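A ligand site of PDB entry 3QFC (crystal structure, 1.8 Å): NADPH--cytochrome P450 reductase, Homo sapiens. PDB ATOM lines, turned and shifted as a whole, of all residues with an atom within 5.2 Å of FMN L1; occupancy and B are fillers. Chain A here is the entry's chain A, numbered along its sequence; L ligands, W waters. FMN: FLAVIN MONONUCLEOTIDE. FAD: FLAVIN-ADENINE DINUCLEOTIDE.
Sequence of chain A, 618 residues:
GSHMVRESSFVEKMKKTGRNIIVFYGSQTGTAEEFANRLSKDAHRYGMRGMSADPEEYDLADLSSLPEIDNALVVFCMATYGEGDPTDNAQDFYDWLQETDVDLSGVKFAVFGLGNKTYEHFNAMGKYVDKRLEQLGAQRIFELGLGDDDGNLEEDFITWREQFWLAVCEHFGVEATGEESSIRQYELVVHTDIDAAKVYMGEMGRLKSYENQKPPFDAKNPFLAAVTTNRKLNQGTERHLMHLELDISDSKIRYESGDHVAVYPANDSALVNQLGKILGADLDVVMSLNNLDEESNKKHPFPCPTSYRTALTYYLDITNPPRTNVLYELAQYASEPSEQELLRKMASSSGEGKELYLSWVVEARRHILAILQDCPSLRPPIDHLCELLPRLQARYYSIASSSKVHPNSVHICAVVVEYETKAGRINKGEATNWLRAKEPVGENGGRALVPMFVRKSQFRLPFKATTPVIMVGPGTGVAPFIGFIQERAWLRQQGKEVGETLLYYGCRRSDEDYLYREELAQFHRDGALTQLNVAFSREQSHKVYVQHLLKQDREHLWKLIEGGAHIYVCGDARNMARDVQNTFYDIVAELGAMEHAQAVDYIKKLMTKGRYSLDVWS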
ATOM      1  N   GLY A  26     -40.604  -4.513  19.527  1.00  0.00           N
ATOM      2  CA  GLY A  26     -40.211  -4.500  18.128  1.00  0.00           C
ATOM      3  C   GLY A  26     -38.798  -5.053  18.245  1.00  0.00           C
ATOM      4  O   GLY A  26     -37.891  -4.331  18.654  1.00  0.00           O
ATOM      5  N   SER A  27     -38.615  -6.317  17.901  1.00  0.00           N
ATOM      6  CA  SER A  27     -37.305  -6.953  18.071  1.00  0.00           C
ATOM      7  C   SER A  27     -36.927  -7.900  16.936  1.00  0.00           C
ATOM      8  O   SER A  27     -37.797  -8.546  16.338  1.00  0.00           O
ATOM      9  CB  SER A  27     -37.348  -7.735  19.398  1.00  0.00           C
ATOM     10  OG  SER A  27     -36.132  -8.394  19.702  1.00  0.00           O
ATOM     11  N   GLN A  28     -35.633  -7.970  16.629  1.00  0.00           N
ATOM     12  CA  GLN A  28     -35.143  -8.862  15.583  1.00  0.00           C
ATOM     13  C   GLN A  28     -34.227  -9.927  16.196  1.00  0.00           C
ATOM     14  O   GLN A  28     -34.288 -11.094  15.806  1.00  0.00           O
ATOM     15  CB  GLN A  28     -34.388  -8.097  14.492  1.00  0.00           C
ATOM     16  CG  GLN A  28     -33.976  -8.979  13.301  1.00  0.00           C
ATOM     17  CD  GLN A  28     -33.435  -8.183  12.126  1.00  0.00           C
ATOM     18  OE1 GLN A  28     -34.138  -7.372  11.522  1.00  0.00           O
ATOM     19  NE2 GLN A  28     -32.169  -8.428  11.783  1.00  0.00           N
ATOM     20  N   THR A  29     -33.373  -9.531  17.142  1.00  0.00           N
ATOM     21  CA  THR A  29     -32.522 -10.508  17.786  1.00  0.00           C
ATOM     22  C   THR A  29     -32.840 -10.741  19.273  1.00  0.00           C
ATOM     23  O   THR A  29     -31.968 -11.099  20.068  1.00  0.00           O
ATOM     24  CB  THR A  29     -31.013 -10.216  17.566  1.00  0.00           C
ATOM     25  OG1 THR A  29     -30.676  -8.905  18.053  1.00  0.00           O
ATOM     26  CG2 THR A  29     -30.689 -10.299  16.071  1.00  0.00           C
ATOM     27  N   GLY A  30     -34.106 -10.525  19.637  1.00  0.00           N
ATOM     28  CA  GLY A  30     -34.574 -10.786  20.987  1.00  0.00           C
ATOM     29  C   GLY A  30     -34.348  -9.852  22.167  1.00  0.00           C
ATOM     30  O   GLY A  30     -34.948 -10.049  23.231  1.00  0.00           O
ATOM     31  N   THR A  31     -33.508  -8.831  22.004  1.00  0.00           N
ATOM     32  CA  THR A  31     -33.217  -7.927  23.109  1.00  0.00           C
ATOM     33  C   THR A  31     -34.439  -7.133  23.545  1.00  0.00           C
ATOM     34  O   THR A  31     -34.737  -7.040  24.739  1.00  0.00           O
ATOM     35  CB  THR A  31     -32.105  -6.932  22.760  1.00  0.00           C
ATOM     36  OG1 THR A  31     -31.057  -7.622  22.070  1.00  0.00           O
ATOM     37  CG2 THR A  31     -31.536  -6.306  24.030  1.00  0.00           C
ATOM     38  N   ALA A  32     -35.161  -6.561  22.581  1.00  0.00           N
ATOM     39  CA  ALA A  32     -36.328  -5.758  22.902  1.00  0.00           C
ATOM     40  C   ALA A  32     -37.403  -6.645  23.546  1.00  0.00           C
ATOM     41  O   ALA A  32     -38.109  -6.198  24.466  1.00  0.00           O
ATOM     42  CB  ALA A  32     -36.881  -5.090  21.635  1.00  0.00           C
ATOM     43  N   GLU A  33     -37.514  -7.886  23.071  1.00  0.00           N
ATOM     44  CA  GLU A  33     -38.502  -8.805  23.644  1.00  0.00           C
ATOM     45  C   GLU A  33     -38.152  -9.075  25.108  1.00  0.00           C
ATOM     46  O   GLU A  33     -39.040  -9.119  25.961  1.00  0.00           O
ATOM     47  CB  GLU A  33     -38.555 -10.130  22.875  1.00  0.00           C
ATOM     48  CG  GLU A  33     -39.529 -11.140  23.501  1.00  0.00           C
ATOM     49  CD  GLU A  33     -39.719 -12.401  22.680  1.00  0.00           C
ATOM     50  OE1 GLU A  33     -40.491 -13.292  23.122  1.00  0.00           O
ATOM     51  OE2 GLU A  33     -39.115 -12.515  21.591  1.00  0.00           O
ATOM     52  N   ALA A  79     -36.754  -1.618  18.780  1.00  0.00           N
ATOM     53  CA  ALA A  79     -35.386  -1.540  18.261  1.00  0.00           C
ATOM     54  C   ALA A  79     -35.432  -0.933  16.869  1.00  0.00           C
ATOM     55  O   ALA A  79     -36.414  -1.094  16.142  1.00  0.00           O
ATOM     56  CB  ALA A  79     -34.756  -2.934  18.183  1.00  0.00           C
ATOM     57  N   THR A  80     -34.360  -0.239  16.498  1.00  0.00           N
ATOM     58  CA  THR A  80     -34.281   0.385  15.175  1.00  0.00           C
ATOM     59  C   THR A  80     -33.352  -0.444  14.281  1.00  0.00           C
ATOM     60  O   THR A  80     -32.305  -0.911  14.734  1.00  0.00           O
ATOM     61  CB  THR A  80     -33.729   1.817  15.256  1.00  0.00           C
ATOM     62  OG1 THR A  80     -34.642   2.649  15.976  1.00  0.00           O
ATOM     63  CG2 THR A  80     -33.518   2.395  13.850  1.00  0.00           C
ATOM     64  N   TYR A  81     -33.730  -0.649  13.030  1.00  0.00           N
ATOM     65  CA  TYR A  81     -32.880  -1.404  12.129  1.00  0.00           C
ATOM     66  C   TYR A  81     -32.538  -0.621  10.866  1.00  0.00           C
ATOM     67  O   TYR A  81     -32.711   0.586  10.809  1.00  0.00           O
ATOM     68  CB  TYR A  81     -33.501  -2.761  11.793  1.00  0.00           C
ATOM     69  CG  TYR A  81     -33.100  -3.809  12.806  1.00  0.00           C
ATOM     70  CD1 TYR A  81     -33.625  -3.810  14.104  1.00  0.00           C
ATOM     71  CD2 TYR A  81     -32.108  -4.749  12.499  1.00  0.00           C
ATOM     72  CE1 TYR A  81     -33.167  -4.718  15.070  1.00  0.00           C
ATOM     73  CE2 TYR A  81     -31.646  -5.645  13.445  1.00  0.00           C
ATOM     74  CZ  TYR A  81     -32.169  -5.628  14.729  1.00  0.00           C
ATOM     75  OH  TYR A  81     -31.687  -6.520  15.661  1.00  0.00           O
ATOM     76  N   GLY A  82     -32.020  -1.331   9.865  1.00  0.00           N
ATOM     77  CA  GLY A  82     -31.622  -0.731   8.614  1.00  0.00           C
ATOM     78  C   GLY A  82     -32.226   0.602   8.196  1.00  0.00           C
ATOM     79  O   GLY A  82     -33.423   0.707   7.956  1.00  0.00           O
ATOM     80  N   GLU A  83     -31.371   1.615   8.127  1.00  0.00           N
ATOM     81  CA  GLU A  83     -31.753   2.959   7.714  1.00  0.00           C
ATOM     82  C   GLU A  83     -32.839   3.607   8.580  1.00  0.00           C
ATOM     83  O   GLU A  83     -33.652   4.398   8.095  1.00  0.00           O
ATOM     84  CB  GLU A  83     -32.212   2.951   6.245  1.00  0.00           C
ATOM     85  CG  GLU A  83     -31.167   2.431   5.237  1.00  0.00           C
ATOM     86  CD  GLU A  83     -30.996   0.913   5.282  1.00  0.00           C
ATOM     87  OE1 GLU A  83     -29.968   0.425   5.810  1.00  0.00           O
ATOM     88  OE2 GLU A  83     -31.890   0.198   4.769  1.00  0.00           O
ATOM     89  N   GLY A  84     -32.840   3.255   9.862  1.00  0.00           N
ATOM     90  CA  GLY A  84     -33.818   3.817  10.795  1.00  0.00           C
ATOM     91  C   GLY A  84     -35.209   3.242  10.646  1.00  0.00           C
ATOM     92  O   GLY A  84     -36.190   3.879  11.034  1.00  0.00           O
ATOM     93  N   THR A  87     -38.324  -3.069  12.967  1.00  0.00           N
ATOM     94  CA  THR A  87     -38.024  -4.487  12.862  1.00  0.00           C
ATOM     95  C   THR A  87     -39.171  -5.054  12.021  1.00  0.00           C
ATOM     96  O   THR A  87     -40.230  -4.419  11.915  1.00  0.00           O
ATOM     97  CB  THR A  87     -38.014  -5.130  14.266  1.00  0.00           C
ATOM     98  OG1 THR A  87     -39.245  -4.825  14.937  1.00  0.00           O
ATOM     99  CG2 THR A  87     -36.855  -4.561  15.081  1.00  0.00           C
ATOM    100  N   LEU A 114     -34.416   0.968  21.520  1.00  0.00           N
ATOM    101  CA  LEU A 114     -33.150   0.253  21.498  1.00  0.00           C
ATOM    102  C   LEU A 114     -32.472   0.693  20.217  1.00  0.00           C
ATOM    103  O   LEU A 114     -33.040   0.566  19.133  1.00  0.00           O
ATOM    104  CB  LEU A 114     -33.368  -1.265  21.435  1.00  0.00           C
ATOM    105  CG  LEU A 114     -33.865  -1.953  22.695  1.00  0.00           C
ATOM    106  CD1 LEU A 114     -35.369  -1.740  22.851  1.00  0.00           C
ATOM    107  CD2 LEU A 114     -33.546  -3.433  22.586  1.00  0.00           C
ATOM    108  N   GLY A 115     -31.252   1.202  20.341  1.00  0.00           N
ATOM    109  CA  GLY A 115     -30.546   1.647  19.169  1.00  0.00           C
ATOM    110  C   GLY A 115     -29.037   1.593  19.366  1.00  0.00           C
ATOM    111  O   GLY A 115     -28.548   0.925  20.274  1.00  0.00           O
ATOM    112  N   ASN A 116     -28.314   2.305  18.508  1.00  0.00           N
ATOM    113  CA  ASN A 116     -26.862   2.311  18.574  1.00  0.00           C
ATOM    114  C   ASN A 116     -26.405   3.608  17.898  1.00  0.00           C
ATOM    115  O   ASN A 116     -26.675   3.834  16.727  1.00  0.00           O
ATOM    116  CB  ASN A 116     -26.324   1.076  17.836  1.00  0.00           C
ATOM    117  CG  ASN A 116     -24.813   0.987  17.874  1.00  0.00           C
ATOM    118  OD1 ASN A 116     -24.115   1.976  17.665  1.00  0.00           O
ATOM    119  ND2 ASN A 116     -24.289  -0.209  18.140  1.00  0.00           N
ATOM    120  N   LYS A 117     -25.718   4.455  18.661  1.00  0.00           N
ATOM    121  CA  LYS A 117     -25.248   5.743  18.141  1.00  0.00           C
ATOM    122  C   LYS A 117     -24.294   5.734  16.960  1.00  0.00           C
ATOM    123  O   LYS A 117     -24.104   6.772  16.332  1.00  0.00           O
ATOM    124  CB  LYS A 117     -24.627   6.579  19.265  1.00  0.00           C
ATOM    125  CG  LYS A 117     -25.642   7.228  20.195  1.00  0.00           C
ATOM    126  CD  LYS A 117     -24.936   7.990  21.314  1.00  0.00           C
ATOM    127  CE  LYS A 117     -25.921   8.757  22.175  1.00  0.00           C
ATOM    128  NZ  LYS A 117     -26.509   9.905  21.411  1.00  0.00           N
ATOM    129  N   TYR A 119     -24.845   4.348  14.243  1.00  0.00           N
ATOM    130  CA  TYR A 119     -25.674   4.384  13.040  1.00  0.00           C
ATOM    131  C   TYR A 119     -26.144   5.795  12.686  1.00  0.00           C
ATOM    132  O   TYR A 119     -26.199   6.677  13.529  1.00  0.00           O
ATOM    133  CB  TYR A 119     -26.876   3.461  13.234  1.00  0.00           C
ATOM    134  CG  TYR A 119     -26.501   2.010  13.170  1.00  0.00           C
ATOM    135  CD1 TYR A 119     -26.314   1.362  11.946  1.00  0.00           C
ATOM    136  CD2 TYR A 119     -26.318   1.269  14.334  1.00  0.00           C
ATOM    137  CE1 TYR A 119     -25.958   0.019  11.890  1.00  0.00           C
ATOM    138  CE2 TYR A 119     -25.955  -0.073  14.289  1.00  0.00           C
ATOM    139  CZ  TYR A 119     -25.779  -0.693  13.069  1.00  0.00           C
ATOM    140  OH  TYR A 119     -25.425  -2.020  13.038  1.00  0.00           O
ATOM    141  N   HIS A 121     -29.201   6.882  11.703  1.00  0.00           N
ATOM    142  CA  HIS A 121     -30.496   7.221  12.285  1.00  0.00           C
ATOM    143  C   HIS A 121     -30.678   6.549  13.649  1.00  0.00           C
ATOM    144  O   HIS A 121     -31.344   5.513  13.783  1.00  0.00           O
ATOM    145  CB  HIS A 121     -31.587   6.776  11.323  1.00  0.00           C
ATOM    146  CG  HIS A 121     -31.473   7.389   9.961  1.00  0.00           C
ATOM    147  ND1 HIS A 121     -31.683   8.730   9.733  1.00  0.00           N
ATOM    148  CD2 HIS A 121     -31.123   6.847   8.769  1.00  0.00           C
ATOM    149  CE1 HIS A 121     -31.458   8.999   8.448  1.00  0.00           C
ATOM    150  NE2 HIS A 121     -31.116   7.869   7.846  1.00  0.00           N
ATOM    151  N   PHE A 122     -30.075   7.164  14.658  1.00  0.00           N
ATOM    152  CA  PHE A 122     -30.099   6.650  16.017  1.00  0.00           C
ATOM    153  C   PHE A 122     -31.483   6.586  16.648  1.00  0.00           C
ATOM    154  O   PHE A 122     -32.169   7.606  16.793  1.00  0.00           O
ATOM    155  CB  PHE A 122     -29.172   7.488  16.887  1.00  0.00           C
ATOM    156  CG  PHE A 122     -29.204   7.131  18.343  1.00  0.00           C
ATOM    157  CD1 PHE A 122     -28.894   5.832  18.756  1.00  0.00           C
ATOM    158  CD2 PHE A 122     -29.546   8.084  19.291  1.00  0.00           C
ATOM    159  CE1 PHE A 122     -28.916   5.500  20.108  1.00  0.00           C
ATOM    160  CE2 PHE A 122     -29.568   7.758  20.652  1.00  0.00           C
ATOM    161  CZ  PHE A 122     -29.261   6.465  21.049  1.00  0.00           C
ATOM    162  N   ASN A 123     -31.899   5.378  17.028  1.00  0.00           N
ATOM    163  CA  ASN A 123     -33.186   5.151  17.683  1.00  0.00           C
ATOM    164  C   ASN A 123     -34.347   5.761  16.913  1.00  0.00           C
ATOM    165  O   ASN A 123     -35.333   6.192  17.508  1.00  0.00           O
ATOM    166  CB  ASN A 123     -33.153   5.732  19.101  1.00  0.00           C
ATOM    167  CG  ASN A 123     -32.904   4.669  20.166  1.00  0.00           C
ATOM    168  OD1 ASN A 123     -32.036   4.839  21.028  1.00  0.00           O
ATOM    169  ND2 ASN A 123     -33.655   3.588  20.106  1.00  0.00           N
ATOM    170  N   ALA A 124     -34.243   5.767  15.588  1.00  0.00           N
ATOM    171  CA  ALA A 124     -35.281   6.347  14.748  1.00  0.00           C
ATOM    172  C   ALA A 124     -36.675   5.753  15.005  1.00  0.00           C
ATOM    173  O   ALA A 124     -37.674   6.493  15.000  1.00  0.00           O
ATOM    174  CB  ALA A 124     -34.914   6.160  13.280  1.00  0.00           C
ATOM    175  N   ASP A 149     -26.664   0.788  22.358  1.00  0.00           N
ATOM    176  CA  ASP A 149     -25.866  -0.440  22.428  1.00  0.00           C
ATOM    177  C   ASP A 149     -24.382  -0.171  22.210  1.00  0.00           C
ATOM    178  O   ASP A 149     -23.549  -1.081  22.364  1.00  0.00           O
ATOM    179  CB  ASP A 149     -26.368  -1.460  21.393  1.00  0.00           C
ATOM    180  CG  ASP A 149     -25.828  -2.863  21.648  1.00  0.00           C
ATOM    181  OD1 ASP A 149     -25.451  -3.546  20.668  1.00  0.00           O
ATOM    182  OD2 ASP A 149     -25.801  -3.292  22.826  1.00  0.00           O
ATOM    183  N   LEU A 153     -26.291  -0.768  26.764  1.00  0.00           N
ATOM    184  CA  LEU A 153     -27.740  -0.779  26.629  1.00  0.00           C
ATOM    185  C   LEU A 153     -28.432  -1.209  27.927  1.00  0.00           C
ATOM    186  O   LEU A 153     -29.441  -0.618  28.322  1.00  0.00           O
ATOM    187  CB  LEU A 153     -28.128  -1.719  25.482  1.00  0.00           C
ATOM    188  CG  LEU A 153     -29.609  -1.847  25.108  1.00  0.00           C
ATOM    189  CD1 LEU A 153     -30.145  -0.502  24.662  1.00  0.00           C
ATOM    190  CD2 LEU A 153     -29.741  -2.875  23.989  1.00  0.00           C
ATOM    191  N   HIS A 260     -27.421  -9.729   3.359  1.00  0.00           N
ATOM    192  CA  HIS A 260     -26.746 -10.380   4.474  1.00  0.00           C
ATOM    193  C   HIS A 260     -27.149 -11.844   4.596  1.00  0.00           C
ATOM    194  O   HIS A 260     -28.285 -12.227   4.263  1.00  0.00           O
ATOM    195  CB  HIS A 260     -27.055  -9.661   5.788  1.00  0.00           C
ATOM    196  CG  HIS A 260     -26.617  -8.226   5.800  1.00  0.00           C
ATOM    197  ND1 HIS A 260     -27.509  -7.179   5.951  1.00  0.00           N
ATOM    198  CD2 HIS A 260     -25.405  -7.653   5.658  1.00  0.00           C
ATOM    199  CE1 HIS A 260     -26.859  -6.028   5.882  1.00  0.00           C
ATOM    200  NE2 HIS A 260     -25.577  -6.294   5.701  1.00  0.00           N
ATOM    201  N   TYR A 396     -24.903 -12.107  11.543  1.00  0.00           N
ATOM    202  CA  TYR A 396     -25.024 -11.678  10.162  1.00  0.00           C
ATOM    203  C   TYR A 396     -23.662 -11.425   9.506  1.00  0.00           C
ATOM    204  O   TYR A 396     -22.749 -10.918  10.144  1.00  0.00           O
ATOM    205  CB  TYR A 396     -25.833 -10.387  10.083  1.00  0.00           C
ATOM    206  CG  TYR A 396     -27.191 -10.458  10.756  1.00  0.00           C
ATOM    207  CD1 TYR A 396     -28.190 -11.303  10.269  1.00  0.00           C
ATOM    208  CD2 TYR A 396     -27.474  -9.681  11.883  1.00  0.00           C
ATOM    209  CE1 TYR A 396     -29.437 -11.371  10.885  1.00  0.00           C
ATOM    210  CE2 TYR A 396     -28.721  -9.743  12.508  1.00  0.00           C
ATOM    211  CZ  TYR A 396     -29.699 -10.591  11.998  1.00  0.00           C
ATOM    212  OH  TYR A 396     -30.930 -10.661  12.630  1.00  0.00           O
HETATM  213  N1  FMN L   1     -29.654   1.250  15.780  1.00  0.00           N
HETATM  214  C2  FMN L   1     -30.008   2.523  15.468  1.00  0.00           C
HETATM  215  O2  FMN L   1     -30.124   3.354  16.358  1.00  0.00           O
HETATM  216  N3  FMN L   1     -30.213   2.849  14.156  1.00  0.00           N
HETATM  217  C4  FMN L   1     -30.078   1.952  13.082  1.00  0.00           C
HETATM  218  O4  FMN L   1     -30.301   2.457  11.974  1.00  0.00           O
HETATM  219  C4A FMN L   1     -29.699   0.589  13.397  1.00  0.00           C
HETATM  220  N5  FMN L   1     -29.561  -0.325  12.323  1.00  0.00           N
HETATM  221  C5A FMN L   1     -29.194  -1.602  12.687  1.00  0.00           C
HETATM  222  C6  FMN L   1     -29.031  -2.541  11.583  1.00  0.00           C
HETATM  223  C7  FMN L   1     -28.665  -3.877  11.792  1.00  0.00           C
HETATM  224  C7M FMN L   1     -28.539  -4.753  10.542  1.00  0.00           C
HETATM  225  C8  FMN L   1     -28.410  -4.370  13.176  1.00  0.00           C
HETATM  226  C8M FMN L   1     -28.006  -5.828  13.511  1.00  0.00           C
HETATM  227  C9  FMN L   1     -28.556  -3.498  14.243  1.00  0.00           C
HETATM  228  C9A FMN L   1     -28.947  -2.096  14.059  1.00  0.00           C
HETATM  229  N10 FMN L   1     -29.115  -1.094  15.143  1.00  0.00           N
HETATM  230  C10 FMN L   1     -29.510   0.307  14.800  1.00  0.00           C
HETATM  231  C1' FMN L   1     -28.892  -1.493  16.520  1.00  0.00           C
HETATM  232  C2' FMN L   1     -30.086  -2.214  17.223  1.00  0.00           C
HETATM  233  O2' FMN L   1     -31.263  -1.360  17.151  1.00  0.00           O
HETATM  234  C3' FMN L   1     -29.713  -2.626  18.655  1.00  0.00           C
HETATM  235  O3' FMN L   1     -28.652  -3.602  18.512  1.00  0.00           O
HETATM  236  C4' FMN L   1     -30.939  -3.289  19.364  1.00  0.00           C
HETATM  237  O4' FMN L   1     -30.448  -3.628  20.701  1.00  0.00           O
HETATM  238  C5' FMN L   1     -31.384  -4.579  18.733  1.00  0.00           C
HETATM  239  O5' FMN L   1     -32.585  -5.120  19.393  1.00  0.00           O
HETATM  240  P   FMN L   1     -33.133  -6.546  19.086  1.00  0.00           P
HETATM  241  O1P FMN L   1     -32.210  -7.599  19.641  1.00  0.00           O
HETATM  242  O2P FMN L   1     -33.452  -6.675  17.649  1.00  0.00           O
HETATM  243  O3P FMN L   1     -34.362  -6.587  19.918  1.00  0.00           O
HETATM  244  PA  FAD L   2     -19.181 -12.993  19.658  1.00  0.00           P
HETATM  245  O1A FAD L   2     -19.090 -14.238  20.474  1.00  0.00           O
HETATM  246  O2A FAD L   2     -20.540 -12.454  19.455  1.00  0.00           O
HETATM  247  O5B FAD L   2     -18.334 -11.982  20.362  1.00  0.00           O
HETATM  248  C5B FAD L   2     -18.159 -10.624  19.911  1.00  0.00           C
HETATM  249  C4B FAD L   2     -17.936  -9.650  21.061  1.00  0.00           C
HETATM  250  O4B FAD L   2     -16.672  -9.971  21.692  1.00  0.00           O
HETATM  251  C3B FAD L   2     -17.771  -8.183  20.653  1.00  0.00           C
HETATM  252  O3B FAD L   2     -19.022  -7.518  20.577  1.00  0.00           O
HETATM  253  C2B FAD L   2     -17.006  -7.597  21.840  1.00  0.00           C
HETATM  254  O2B FAD L   2     -17.810  -7.232  22.997  1.00  0.00           O
HETATM  255  C1B FAD L   2     -16.069  -8.764  22.195  1.00  0.00           C
HETATM  256  N9A FAD L   2     -14.690  -8.678  21.659  1.00  0.00           N
HETATM  257  C8A FAD L   2     -14.120  -8.974  20.428  1.00  0.00           C
HETATM  258  N7A FAD L   2     -12.761  -8.750  20.358  1.00  0.00           N
HETATM  259  C5A FAD L   2     -12.452  -8.289  21.607  1.00  0.00           C
HETATM  260  C6A FAD L   2     -11.230  -7.855  22.252  1.00  0.00           C
HETATM  261  N6A FAD L   2     -10.022  -7.859  21.611  1.00  0.00           N
HETATM  262  N1A FAD L   2     -11.359  -7.444  23.586  1.00  0.00           N
HETATM  263  C2A FAD L   2     -12.502  -7.399  24.325  1.00  0.00           C
HETATM  264  N3A FAD L   2     -13.723  -7.785  23.818  1.00  0.00           N
HETATM  265  C4A FAD L   2     -13.641  -8.229  22.443  1.00  0.00           C
HETATM  266  N1  FAD L   2     -18.197  -9.814  10.513  1.00  0.00           N
HETATM  267  C2  FAD L   2     -17.296 -10.267   9.584  1.00  0.00           C
HETATM  268  O2  FAD L   2     -16.251 -10.781   9.984  1.00  0.00           O
HETATM  269  N3  FAD L   2     -17.633 -10.124   8.272  1.00  0.00           N
HETATM  270  C4  FAD L   2     -18.823  -9.542   7.730  1.00  0.00           C
HETATM  271  O4  FAD L   2     -19.004  -9.470   6.501  1.00  0.00           O
HETATM  272  C4X FAD L   2     -19.748  -9.047   8.737  1.00  0.00           C
HETATM  273  N5  FAD L   2     -20.907  -8.454   8.250  1.00  0.00           N
HETATM  274  C5X FAD L   2     -21.788  -7.980   9.214  1.00  0.00           C
HETATM  275  C6  FAD L   2     -23.004  -7.338   8.751  1.00  0.00           C
HETATM  276  C7  FAD L   2     -23.989  -6.830   9.661  1.00  0.00           C
HETATM  277  C7M FAD L   2     -25.256  -6.175   9.135  1.00  0.00           C
HETATM  278  C8  FAD L   2     -23.721  -6.969  11.113  1.00  0.00           C
HETATM  279  C8M FAD L   2     -24.677  -6.473  12.193  1.00  0.00           C
HETATM  280  C9  FAD L   2     -22.567  -7.580  11.589  1.00  0.00           C
HETATM  281  C9A FAD L   2     -21.566  -8.091  10.694  1.00  0.00           C
HETATM  282  N10 FAD L   2     -20.306  -8.754  11.114  1.00  0.00           N
HETATM  283  C10 FAD L   2     -19.400  -9.212  10.140  1.00  0.00           C
HETATM  284  C1' FAD L   2     -19.916  -8.976  12.547  1.00  0.00           C
HETATM  285  C2' FAD L   2     -20.622 -10.424  12.689  1.00  0.00           C
HETATM  286  O2' FAD L   2     -22.127 -10.457  12.627  1.00  0.00           O
HETATM  287  C3' FAD L   2     -20.286 -10.926  14.182  1.00  0.00           C
HETATM  288  O3' FAD L   2     -20.670  -9.951  15.199  1.00  0.00           O
HETATM  289  C4' FAD L   2     -18.796 -11.253  14.426  1.00  0.00           C
HETATM  290  O4' FAD L   2     -18.429 -12.214  13.410  1.00  0.00           O
HETATM  291  C5' FAD L   2     -18.500 -11.762  15.750  1.00  0.00           C
HETATM  292  O5' FAD L   2     -19.358 -12.804  16.209  1.00  0.00           O
HETATM  293  P   FAD L   2     -18.941 -13.948  17.095  1.00  0.00           P
HETATM  294  O1P FAD L   2     -17.818 -14.765  16.524  1.00  0.00           O
HETATM  295  O2P FAD L   2     -20.191 -14.721  17.304  1.00  0.00           O
HETATM  296  O3P FAD L   2     -18.459 -13.091  18.344  1.00  0.00           O
HETATM  297  O   HOH W   1     -28.929   0.980   9.601  1.00  0.00           O
HETATM  298  O   HOH W   2     -26.071  -2.610  18.346  1.00  0.00           O
HETATM  299  O   HOH W   3     -28.855  -5.726  21.423  1.00  0.00           O
HETATM  300  O   HOH W   4     -29.166   4.387  10.309  1.00  0.00           O
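The side-chain hydroxyl (OG) of Ser 27 lies within hydrogen-bond range of an oxygen (O3P) of FMN L1.
The backbone NH of Thr 29 sits at hydrogen-bond distance from an oxygen (O2P) of FMN L1, at 2.9 Å.
An oxygen (O1P) of FMN L1 sits at hydrogen-bond distance from the side-chain hydroxyl (OG1) of Thr 29 (2.6 Å).
The side-chain hydroxyl of Tyr 81 is in hydrogen-bond range of an oxygen (O2P) of FMN L1.
The backbone NH (N) of Thr 80 lies within hydrogen-bond range of an oxygen (O2') of FMN L1.
The backbone carbonyl oxygen (O) of Thr 80 is in hydrogen-bond range of an oxygen (O2') of FMN L1 (2.7 Å).
The backbone NH (N) of Thr 31 sits at hydrogen-bond distance from an oxygen (O1P) of FMN L1.
OG1 of Thr 31 lies within hydrogen-bond range of O1P of FMN L1 (2.7 Å).
The backbone NH (N) of Gln 28 sits at hydrogen-bond distance from an oxygen (O2P) of FMN L1 (2.7 Å).
O2 of FMN L1 is in hydrogen-bond range of N of Asn 123, at 2.8 Å.
An oxygen (O3P) of FMN L1 is in hydrogen-bond range of the backbone NH (N) of Ala 32.
The backbone carbonyl oxygen (O) of His 121 sits at hydrogen-bond distance from a nitrogen (N3) of FMN L1 (2.9 Å).
An oxygen (O2) of FMN L1 lies within hydrogen-bond range of the backbone NH (N) of Asn 116 (3.0 Å).
An oxygen (O2') of FMN L1 is in hydrogen-bond range of the backbone carbonyl oxygen (O) of Leu 114.
N of Gly 84 lies within hydrogen-bond range of O4 of FMN L1 (3.4 Å).
O1P of FMN L1 is in hydrogen-bond range of N of Gly 30, at 3.5 Å.
N of Tyr 396 is in hydrogen-bond range of O2' of FAD L2 (3.4 Å).
O of Tyr 396 lies within hydrogen-bond range of O2' of FAD L2, at 2.6 Å.
The side-chain hydroxyl (OG) of Ser 27 lies within hydrogen-bond range of the backbone NH (N) of Gly 30 (2.9 Å).
N of Ser 27 sits at hydrogen-bond distance from OG1 of Thr 87 (3.4 Å).
The backbone NH of Thr 80 lies within hydrogen-bond range of the backbone carbonyl oxygen of Leu 114 (3.1 Å).
N of Ala 124 is in hydrogen-bond range of OG1 of Thr 80 (3.2 Å).
The backbone NH (N) of Leu 114 lies close to the side-chain amide nitrogen (ND2) of Asn 123, at 3.1 Å.
The backbone NH (N) of Gly 115 lies close to the side-chain amide nitrogen (ND2) of Asn 123 (3.4 Å).
N of Ala 79 is in hydrogen-bond range of O of Gly 26 (2.9 Å).
The backbone carbonyl oxygen (O) of Gly 115 sits at hydrogen-bond distance from the backbone NH (N) of Asp 149 (2.8 Å).
Merely in contact with FMN L1: Ala 79 (3.3 Å), Gly 82 (3.6 Å), Gly 115 (3.3 Å), Tyr 119 (3.4 Å), Phe 122 (3.3 Å), Asp 149 (3.9 Å) and Leu 153 (3.4 Å).
Hydrophobic or aromatic side chains within 4 Å of FMN L1: Ala 32, Ala 79, Tyr 81, Leu 114, Tyr 119, Phe 122 and Leu 153.
20 residues have an atom within 4 Å of FMN L1: Ser 27, Gln 28, Thr 29, Gly 30, Thr 31, Ala 32, Ala 79, Thr 80, Tyr 81, Gly 82, Gly 84, Leu 114, Gly 115, Asn 116, Tyr 119, His 121, Phe 122, Asn 123, Asp 149 and Leu 153.
Along chain A the residues within 4 Å of FMN L1 span positions 27 to 153.
Water W3 bridges O4' of FMN L1 and OG1 of Thr 31.
Water W2 lies within hydrogen-bond range of the side-chain carboxylate (OD1) of Asp 149 (2.6 Å), an oxygen (O3') of FMN L1 (2.8 Å) and the side-chain amide nitrogen (ND2) of Asn 116 (3.0 Å).
Water W4 bridges O4 of FMN L1 (2.8 Å) and N of His 121 (2.9 Å).
Water W1 lies within hydrogen-bond range of the backbone NH of Glu 83 (2.9 Å) and a nitrogen (N5) of FMN L1 (3.1 Å).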
